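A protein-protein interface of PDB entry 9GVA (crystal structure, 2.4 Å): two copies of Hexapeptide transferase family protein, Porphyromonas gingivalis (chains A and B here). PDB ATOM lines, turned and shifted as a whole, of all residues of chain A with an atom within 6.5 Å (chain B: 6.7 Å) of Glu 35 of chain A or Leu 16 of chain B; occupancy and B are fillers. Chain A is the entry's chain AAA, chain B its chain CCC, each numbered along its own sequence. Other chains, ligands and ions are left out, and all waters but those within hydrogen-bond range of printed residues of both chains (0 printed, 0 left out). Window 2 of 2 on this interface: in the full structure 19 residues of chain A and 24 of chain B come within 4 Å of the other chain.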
ATOM      1  N   LYS A  13     -21.591  21.907 -22.587  1.00  0.00           N
ATOM      2  CA  LYS A  13     -20.969  20.996 -23.600  1.00  0.00           C
ATOM      3  C   LYS A  13     -21.979  20.689 -24.714  1.00  0.00           C
ATOM      4  O   LYS A  13     -21.703  21.116 -25.857  1.00  0.00           O
ATOM      5  CB  LYS A  13     -20.506  19.655 -23.011  1.00  0.00           C
ATOM      6  CG  LYS A  13     -19.298  19.684 -22.085  1.00  0.00           C
ATOM      7  CD  LYS A  13     -18.812  18.289 -21.741  1.00  0.00           C
ATOM      8  CE  LYS A  13     -18.036  18.231 -20.444  1.00  0.00           C
ATOM      9  NZ  LYS A  13     -17.024  19.313 -20.369  1.00  0.00           N
ATOM     10  N   MET A  14     -23.061  19.936 -24.422  1.00  0.00           N
ATOM     11  CA  MET A  14     -23.958  19.398 -25.483  1.00  0.00           C
ATOM     12  C   MET A  14     -25.444  19.372 -25.049  1.00  0.00           C
ATOM     13  O   MET A  14     -25.760  19.404 -23.850  1.00  0.00           O
ATOM     14  CB  MET A  14     -23.451  18.031 -25.977  1.00  0.00           C
ATOM     15  CG  MET A  14     -24.101  16.801 -25.343  1.00  0.00           C
ATOM     16  SD  MET A  14     -24.373  15.392 -26.511  1.00  0.00           S
ATOM     17  CE  MET A  14     -25.493  16.052 -27.750  1.00  0.00           C
ATOM     18  N   ALA A  15     -26.352  19.317 -26.025  1.00  0.00           N
ATOM     19  CA  ALA A  15     -27.815  19.203 -25.819  1.00  0.00           C
ATOM     20  C   ALA A  15     -28.108  18.068 -24.835  1.00  0.00           C
ATOM     21  O   ALA A  15     -27.460  17.041 -24.928  1.00  0.00           O
ATOM     22  CB  ALA A  15     -28.525  18.971 -27.136  1.00  0.00           C
ATOM     23  N   LEU A  16     -29.092  18.260 -23.956  1.00  0.00           N
ATOM     24  CA  LEU A  16     -29.646  17.216 -23.077  1.00  0.00           C
ATOM     25  C   LEU A  16     -30.469  16.241 -23.934  1.00  0.00           C
ATOM     26  O   LEU A  16     -31.515  16.635 -24.505  1.00  0.00           O
ATOM     27  CB  LEU A  16     -30.495  17.889 -22.003  1.00  0.00           C
ATOM     28  CG  LEU A  16     -31.188  16.921 -21.057  1.00  0.00           C
ATOM     29  CD1 LEU A  16     -30.173  15.956 -20.425  1.00  0.00           C
ATOM     30  CD2 LEU A  16     -31.985  17.686 -20.019  1.00  0.00           C
ATOM     31  N   PHE A  32     -28.254  20.415 -36.523  1.00  0.00           N
ATOM     32  CA  PHE A  32     -27.714  21.251 -35.434  1.00  0.00           C
ATOM     33  C   PHE A  32     -28.634  21.174 -34.187  1.00  0.00           C
ATOM     34  O   PHE A  32     -29.860  21.383 -34.283  1.00  0.00           O
ATOM     35  CB  PHE A  32     -27.549  22.669 -35.969  1.00  0.00           C
ATOM     36  CG  PHE A  32     -27.310  23.684 -34.879  1.00  0.00           C
ATOM     37  CD1 PHE A  32     -26.113  23.705 -34.190  1.00  0.00           C
ATOM     38  CD2 PHE A  32     -28.297  24.592 -34.521  1.00  0.00           C
ATOM     39  CE1 PHE A  32     -25.903  24.626 -33.167  1.00  0.00           C
ATOM     40  CE2 PHE A  32     -28.079  25.508 -33.510  1.00  0.00           C
ATOM     41  CZ  PHE A  32     -26.888  25.515 -32.820  1.00  0.00           C
ATOM     42  N   LEU A  33     -28.065  20.838 -33.035  1.00  0.00           N
ATOM     43  CA  LEU A  33     -28.726  20.913 -31.705  1.00  0.00           C
ATOM     44  C   LEU A  33     -28.008  21.941 -30.833  1.00  0.00           C
ATOM     45  O   LEU A  33     -26.865  21.701 -30.502  1.00  0.00           O
ATOM     46  CB  LEU A  33     -28.666  19.541 -31.034  1.00  0.00           C
ATOM     47  CG  LEU A  33     -29.306  18.384 -31.806  1.00  0.00           C
ATOM     48  CD1 LEU A  33     -29.235  17.114 -30.992  1.00  0.00           C
ATOM     49  CD2 LEU A  33     -30.746  18.663 -32.205  1.00  0.00           C
ATOM     50  N   ALA A  34     -28.655  23.028 -30.432  1.00  0.00           N
ATOM     51  CA  ALA A  34     -28.042  23.976 -29.478  1.00  0.00           C
ATOM     52  C   ALA A  34     -27.642  23.216 -28.194  1.00  0.00           C
ATOM     53  O   ALA A  34     -28.281  22.188 -27.823  1.00  0.00           O
ATOM     54  CB  ALA A  34     -28.962  25.147 -29.223  1.00  0.00           C
ATOM     55  N   GLU A  35     -26.597  23.714 -27.548  1.00  0.00           N
ATOM     56  CA  GLU A  35     -25.977  23.206 -26.292  1.00  0.00           C
ATOM     57  C   GLU A  35     -26.996  23.028 -25.176  1.00  0.00           C
ATOM     58  O   GLU A  35     -26.727  22.177 -24.346  1.00  0.00           O
ATOM     59  CB  GLU A  35     -24.933  24.200 -25.770  1.00  0.00           C
ATOM     60  CG  GLU A  35     -23.510  23.753 -26.053  1.00  0.00           C
ATOM     61  CD  GLU A  35     -22.530  24.842 -26.477  1.00  0.00           C
ATOM     62  OE1 GLU A  35     -22.267  24.946 -27.700  1.00  0.00           O
ATOM     63  OE2 GLU A  35     -22.014  25.568 -25.594  1.00  0.00           O
ATOM     64  N   ASN A  36     -28.036  23.873 -25.116  1.00  0.00           N
ATOM     65  CA  ASN A  36     -29.024  23.918 -24.009  1.00  0.00           C
ATOM     66  C   ASN A  36     -30.410  23.555 -24.574  1.00  0.00           C
ATOM     67  O   ASN A  36     -31.429  23.906 -23.961  1.00  0.00           O
ATOM     68  CB  ASN A  36     -28.957  25.293 -23.335  1.00  0.00           C
ATOM     69  CG  ASN A  36     -29.132  26.441 -24.319  1.00  0.00           C
ATOM     70  OD1 ASN A  36     -29.692  26.270 -25.395  1.00  0.00           O
ATOM     71  ND2 ASN A  36     -28.656  27.624 -23.972  1.00  0.00           N
ATOM     72  N   ALA A  37     -30.459  22.904 -25.733  1.00  0.00           N
ATOM     73  CA  ALA A  37     -31.695  22.279 -26.240  1.00  0.00           C
ATOM     74  C   ALA A  37     -31.963  20.998 -25.450  1.00  0.00           C
ATOM     75  O   ALA A  37     -31.042  20.419 -24.881  1.00  0.00           O
ATOM     76  CB  ALA A  37     -31.580  22.022 -27.724  1.00  0.00           C
ATOM     77  N   VAL A  51     -32.292  22.936 -34.015  1.00  0.00           N
ATOM     78  CA  VAL A  51     -33.008  23.034 -32.725  1.00  0.00           C
ATOM     79  C   VAL A  51     -32.228  24.053 -31.914  1.00  0.00           C
ATOM     80  O   VAL A  51     -31.098  23.789 -31.498  1.00  0.00           O
ATOM     81  CB  VAL A  51     -33.118  21.685 -32.002  1.00  0.00           C
ATOM     82  CG1 VAL A  51     -33.884  21.812 -30.693  1.00  0.00           C
ATOM     83  CG2 VAL A  51     -33.714  20.602 -32.895  1.00  0.00           C
ATOM     84  N   TRP A  52     -32.856  25.184 -31.691  1.00  0.00           N
ATOM     85  CA  TRP A  52     -32.199  26.377 -31.145  1.00  0.00           C
ATOM     86  C   TRP A  52     -32.260  26.383 -29.621  1.00  0.00           C
ATOM     87  O   TRP A  52     -32.680  25.386 -29.008  1.00  0.00           O
ATOM     88  CB  TRP A  52     -32.804  27.591 -31.828  1.00  0.00           C
ATOM     89  CG  TRP A  52     -32.266  27.709 -33.220  1.00  0.00           C
ATOM     90  CD1 TRP A  52     -32.879  27.327 -34.381  1.00  0.00           C
ATOM     91  CD2 TRP A  52     -30.961  28.196 -33.590  1.00  0.00           C
ATOM     92  NE1 TRP A  52     -32.057  27.566 -35.445  1.00  0.00           N
ATOM     93  CE2 TRP A  52     -30.878  28.108 -35.000  1.00  0.00           C
ATOM     94  CE3 TRP A  52     -29.867  28.722 -32.876  1.00  0.00           C
ATOM     95  CZ2 TRP A  52     -29.744  28.528 -35.713  1.00  0.00           C
ATOM     96  CZ3 TRP A  52     -28.745  29.135 -33.581  1.00  0.00           C
ATOM     97  CH2 TRP A  52     -28.686  29.023 -34.977  1.00  0.00           C
ATOM     98  N   PHE A  53     -31.712  27.453 -29.059  1.00  0.00           N
ATOM     99  CA  PHE A  53     -31.412  27.600 -27.625  1.00  0.00           C
ATOM    100  C   PHE A  53     -32.691  27.360 -26.827  1.00  0.00           C
ATOM    101  O   PHE A  53     -33.728  27.983 -27.124  1.00  0.00           O
ATOM    102  CB  PHE A  53     -30.814  28.993 -27.411  1.00  0.00           C
ATOM    103  CG  PHE A  53     -29.479  29.157 -28.084  1.00  0.00           C
ATOM    104  CD1 PHE A  53     -28.400  28.373 -27.700  1.00  0.00           C
ATOM    105  CD2 PHE A  53     -29.306  30.065 -29.117  1.00  0.00           C
ATOM    106  CE1 PHE A  53     -27.177  28.485 -28.350  1.00  0.00           C
ATOM    107  CE2 PHE A  53     -28.080  30.179 -29.760  1.00  0.00           C
ATOM    108  CZ  PHE A  53     -27.016  29.393 -29.372  1.00  0.00           C
ATOM    109  N   MET B  14     -21.259  29.145 -16.019  1.00  0.00           N
ATOM    110  CA  MET B  14     -21.699  30.527 -16.357  1.00  0.00           C
ATOM    111  C   MET B  14     -22.482  30.571 -17.688  1.00  0.00           C
ATOM    112  O   MET B  14     -22.740  29.522 -18.313  1.00  0.00           O
ATOM    113  CB  MET B  14     -20.511  31.496 -16.354  1.00  0.00           C
ATOM    114  CG  MET B  14     -19.452  31.197 -17.374  1.00  0.00           C
ATOM    115  SD  MET B  14     -18.504  32.694 -17.789  1.00  0.00           S
ATOM    116  CE  MET B  14     -19.594  33.504 -18.965  1.00  0.00           C
ATOM    117  N   ALA B  15     -22.940  31.766 -18.046  1.00  0.00           N
ATOM    118  CA  ALA B  15     -23.746  32.076 -19.243  1.00  0.00           C
ATOM    119  C   ALA B  15     -23.040  31.531 -20.487  1.00  0.00           C
ATOM    120  O   ALA B  15     -21.816  31.635 -20.578  1.00  0.00           O
ATOM    121  CB  ALA B  15     -23.949  33.565 -19.334  1.00  0.00           C
ATOM    122  N   LEU B  16     -23.806  30.960 -21.410  1.00  0.00           N
ATOM    123  CA  LEU B  16     -23.321  30.579 -22.748  1.00  0.00           C
ATOM    124  C   LEU B  16     -23.084  31.873 -23.536  1.00  0.00           C
ATOM    125  O   LEU B  16     -24.059  32.555 -23.866  1.00  0.00           O
ATOM    126  CB  LEU B  16     -24.357  29.663 -23.390  1.00  0.00           C
ATOM    127  CG  LEU B  16     -23.989  29.126 -24.767  1.00  0.00           C
ATOM    128  CD1 LEU B  16     -22.580  28.592 -24.761  1.00  0.00           C
ATOM    129  CD2 LEU B  16     -24.961  28.049 -25.202  1.00  0.00           C
ATOM    130  N   ILE B  17     -21.817  32.253 -23.722  1.00  0.00           N
ATOM    131  CA  ILE B  17     -21.414  33.393 -24.599  1.00  0.00           C
ATOM    132  C   ILE B  17     -20.644  32.819 -25.791  1.00  0.00           C
ATOM    133  O   ILE B  17     -19.736  32.061 -25.575  1.00  0.00           O
ATOM    134  CB  ILE B  17     -20.596  34.427 -23.813  1.00  0.00           C
ATOM    135  CG1 ILE B  17     -21.386  35.008 -22.642  1.00  0.00           C
ATOM    136  CG2 ILE B  17     -20.123  35.525 -24.743  1.00  0.00           C
ATOM    137  CD1 ILE B  17     -20.533  35.602 -21.574  1.00  0.00           C
ATOM    138  N   GLN B  18     -21.043  33.108 -27.022  1.00  0.00           N
ATOM    139  CA  GLN B  18     -20.415  32.529 -28.234  1.00  0.00           C
ATOM    140  C   GLN B  18     -20.306  33.614 -29.287  1.00  0.00           C
ATOM    141  O   GLN B  18     -21.179  34.483 -29.294  1.00  0.00           O
ATOM    142  CB  GLN B  18     -21.242  31.395 -28.844  1.00  0.00           C
ATOM    143  CG  GLN B  18     -21.468  30.217 -27.912  1.00  0.00           C
ATOM    144  CD  GLN B  18     -22.054  29.028 -28.641  1.00  0.00           C
ATOM    145  OE1 GLN B  18     -22.839  29.168 -29.578  1.00  0.00           O
ATOM    146  NE2 GLN B  18     -21.702  27.835 -28.182  1.00  0.00           N
ATOM    147  N   ALA B  34     -27.228  35.698 -15.787  1.00  0.00           N
ATOM    148  CA  ALA B  34     -27.635  34.430 -15.159  1.00  0.00           C
ATOM    149  C   ALA B  34     -26.791  33.306 -15.765  1.00  0.00           C
ATOM    150  O   ALA B  34     -26.439  33.340 -16.963  1.00  0.00           O
ATOM    151  CB  ALA B  34     -29.106  34.186 -15.362  1.00  0.00           C
ATOM    152  N   GLU B  35     -26.505  32.290 -14.984  1.00  0.00           N
ATOM    153  CA  GLU B  35     -25.604  31.233 -15.486  1.00  0.00           C
ATOM    154  C   GLU B  35     -26.282  30.383 -16.571  1.00  0.00           C
ATOM    155  O   GLU B  35     -25.547  29.629 -17.204  1.00  0.00           O
ATOM    156  CB  GLU B  35     -25.094  30.398 -14.318  1.00  0.00           C
ATOM    157  CG  GLU B  35     -26.179  29.733 -13.513  1.00  0.00           C
ATOM    158  CD  GLU B  35     -25.591  29.292 -12.190  1.00  0.00           C
ATOM    159  OE1 GLU B  35     -25.248  28.076 -12.084  1.00  0.00           O
ATOM    160  OE2 GLU B  35     -25.407  30.188 -11.301  1.00  0.00           O
ATOM    161  N   ASN B  36     -27.606  30.475 -16.801  1.00  0.00           N
ATOM    162  CA  ASN B  36     -28.260  29.730 -17.919  1.00  0.00           C
ATOM    163  C   ASN B  36     -28.778  30.734 -18.965  1.00  0.00           C
ATOM    164  O   ASN B  36     -29.610  30.356 -19.769  1.00  0.00           O
ATOM    165  CB  ASN B  36     -29.322  28.747 -17.423  1.00  0.00           C
ATOM    166  CG  ASN B  36     -30.332  29.427 -16.519  1.00  0.00           C
ATOM    167  OD1 ASN B  36     -30.501  30.649 -16.597  1.00  0.00           O
ATOM    168  ND2 ASN B  36     -30.933  28.672 -15.616  1.00  0.00           N
ATOM    169  N   ALA B  37     -28.288  31.974 -18.966  1.00  0.00           N
ATOM    170  CA  ALA B  37     -28.496  32.930 -20.070  1.00  0.00           C
ATOM    171  C   ALA B  37     -27.604  32.514 -21.243  1.00  0.00           C
ATOM    172  O   ALA B  37     -26.648  31.740 -21.063  1.00  0.00           O
ATOM    173  CB  ALA B  37     -28.244  34.360 -19.660  1.00  0.00           C
ATOM    174  N   THR B  38     -28.009  32.951 -22.421  1.00  0.00           N
ATOM    175  CA  THR B  38     -27.339  32.712 -23.702  1.00  0.00           C
ATOM    176  C   THR B  38     -27.157  34.090 -24.314  1.00  0.00           C
ATOM    177  O   THR B  38     -28.169  34.815 -24.470  1.00  0.00           O
ATOM    178  CB  THR B  38     -28.154  31.756 -24.579  1.00  0.00           C
ATOM    179  OG1 THR B  38     -28.272  30.480 -23.928  1.00  0.00           O
ATOM    180  CG2 THR B  38     -27.555  31.597 -25.956  1.00  0.00           C
ATOM    181  N   ILE B  39     -25.921  34.441 -24.637  1.00  0.00           N
ATOM    182  CA  ILE B  39     -25.606  35.654 -25.451  1.00  0.00           C
ATOM    183  C   ILE B  39     -24.628  35.245 -26.548  1.00  0.00           C
ATOM    184  O   ILE B  39     -23.497  34.823 -26.257  1.00  0.00           O
ATOM    185  CB  ILE B  39     -25.054  36.833 -24.627  1.00  0.00           C
ATOM    186  CG1 ILE B  39     -25.812  37.083 -23.328  1.00  0.00           C
ATOM    187  CG2 ILE B  39     -25.041  38.066 -25.485  1.00  0.00           C
ATOM    188  CD1 ILE B  39     -25.340  36.195 -22.212  1.00  0.00           C
ATOM    189  N   VAL B  40     -25.009  35.512 -27.769  1.00  0.00           N
ATOM    190  CA  VAL B  40     -24.349  34.915 -28.947  1.00  0.00           C
ATOM    191  C   VAL B  40     -24.238  35.965 -30.066  1.00  0.00           C
ATOM    192  O   VAL B  40     -25.193  36.695 -30.309  1.00  0.00           O
ATOM    193  CB  VAL B  40     -25.210  33.683 -29.256  1.00  0.00           C
ATOM    194  CG1 VAL B  40     -25.626  33.561 -30.695  1.00  0.00           C
ATOM    195  CG2 VAL B  40     -24.585  32.417 -28.681  1.00  0.00           C
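Of the 12 printed residues of chain B, 4 touch a printed residue of chain A. Hydrophobic or aromatic side chains of chain B that line the printed part of chain A: Leu 16 and Val 40. Among the printed residues, no Asp or Glu carboxylate lies within 4 Å of a Lys or Arg side-chain nitrogen of the other chain.
Printed residues of chain B within 4 Å of Glu 35 of chain A: Leu 16 (3.2 Å) and Gln 18 (3.0 Å). Printed residues of chain B within 4 Å of Asn 36 of chain A: Leu 16 and Thr 38. Of chain A, only Glu 35 (3.2 Å), Asn 36 (3.9 Å) and Phe 53 (3.9 Å) come within 4 Å of Leu 16 of chain B. Ile 17 of chain B touches none of the printed residues of chain A. Ala 37 of chain B touches none of the printed residues of chain A. Of the printed residues of chain A, Val 40 of chain B touches Phe 53. The nearest printed residue of chain A that does not touch Val 40 of chain B is Trp 52 of chain A (6.1 Å).
Glu 35 of chain A touches Leu 16 of chain B, but with the chains exchanged Leu 16 of chain A does not touch Glu 35 of chain B (13.6 Å). Asn 36 of chain A touches Leu 16 of chain B, but with the chains exchanged Leu 16 of chain A does not touch Asn 36 of chain B (11.7 Å). Positions printed for both chains: 14, 15, 16, 34, 35, 36 and 37.
Among the printed residues, merely in contact across the chains: Glu 35 of chain A with Leu 16 of chain B (3.2 Å), Asn 36 of chain A with Leu 16 of chain B (3.9 Å), Phe 53 of chain A with Leu 16 of chain B (3.9 Å), Phe 53 of chain A with Thr 38 of chain B (3.8 Å) and Phe 53 of chain A with Val 40 of chain B (3.9 Å).
The side-chain amide nitrogen (NE2) of Gln 18 of chain B sits at hydrogen-bond distance from the side-chain carboxylate (OE1) of Glu 35 of chain A (3.0 Å). ND2 of Asn 36 of chain A lies within hydrogen-bond range of OG1 of Thr 38 of chain B, 2.9 Å away.
The backbone carbonyl oxygen (O) of Ile 39 of chain B is in hydrogen-bond range of the backbone NH (N) of Gln 18 of chain B (3.1 Å). The backbone carbonyl oxygen (O) of Leu 16 of chain B sits at hydrogen-bond distance from the backbone NH (N) of Ile 39 of chain B (2.8 Å). O of Ala 37 of chain B sits at hydrogen-bond distance from N of Leu 16 of chain B. The backbone carbonyl oxygen (O) of Glu 35 of chain A sits at hydrogen-bond distance from the backbone NH (N) of Ala 15 of chain A (3.3 Å).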
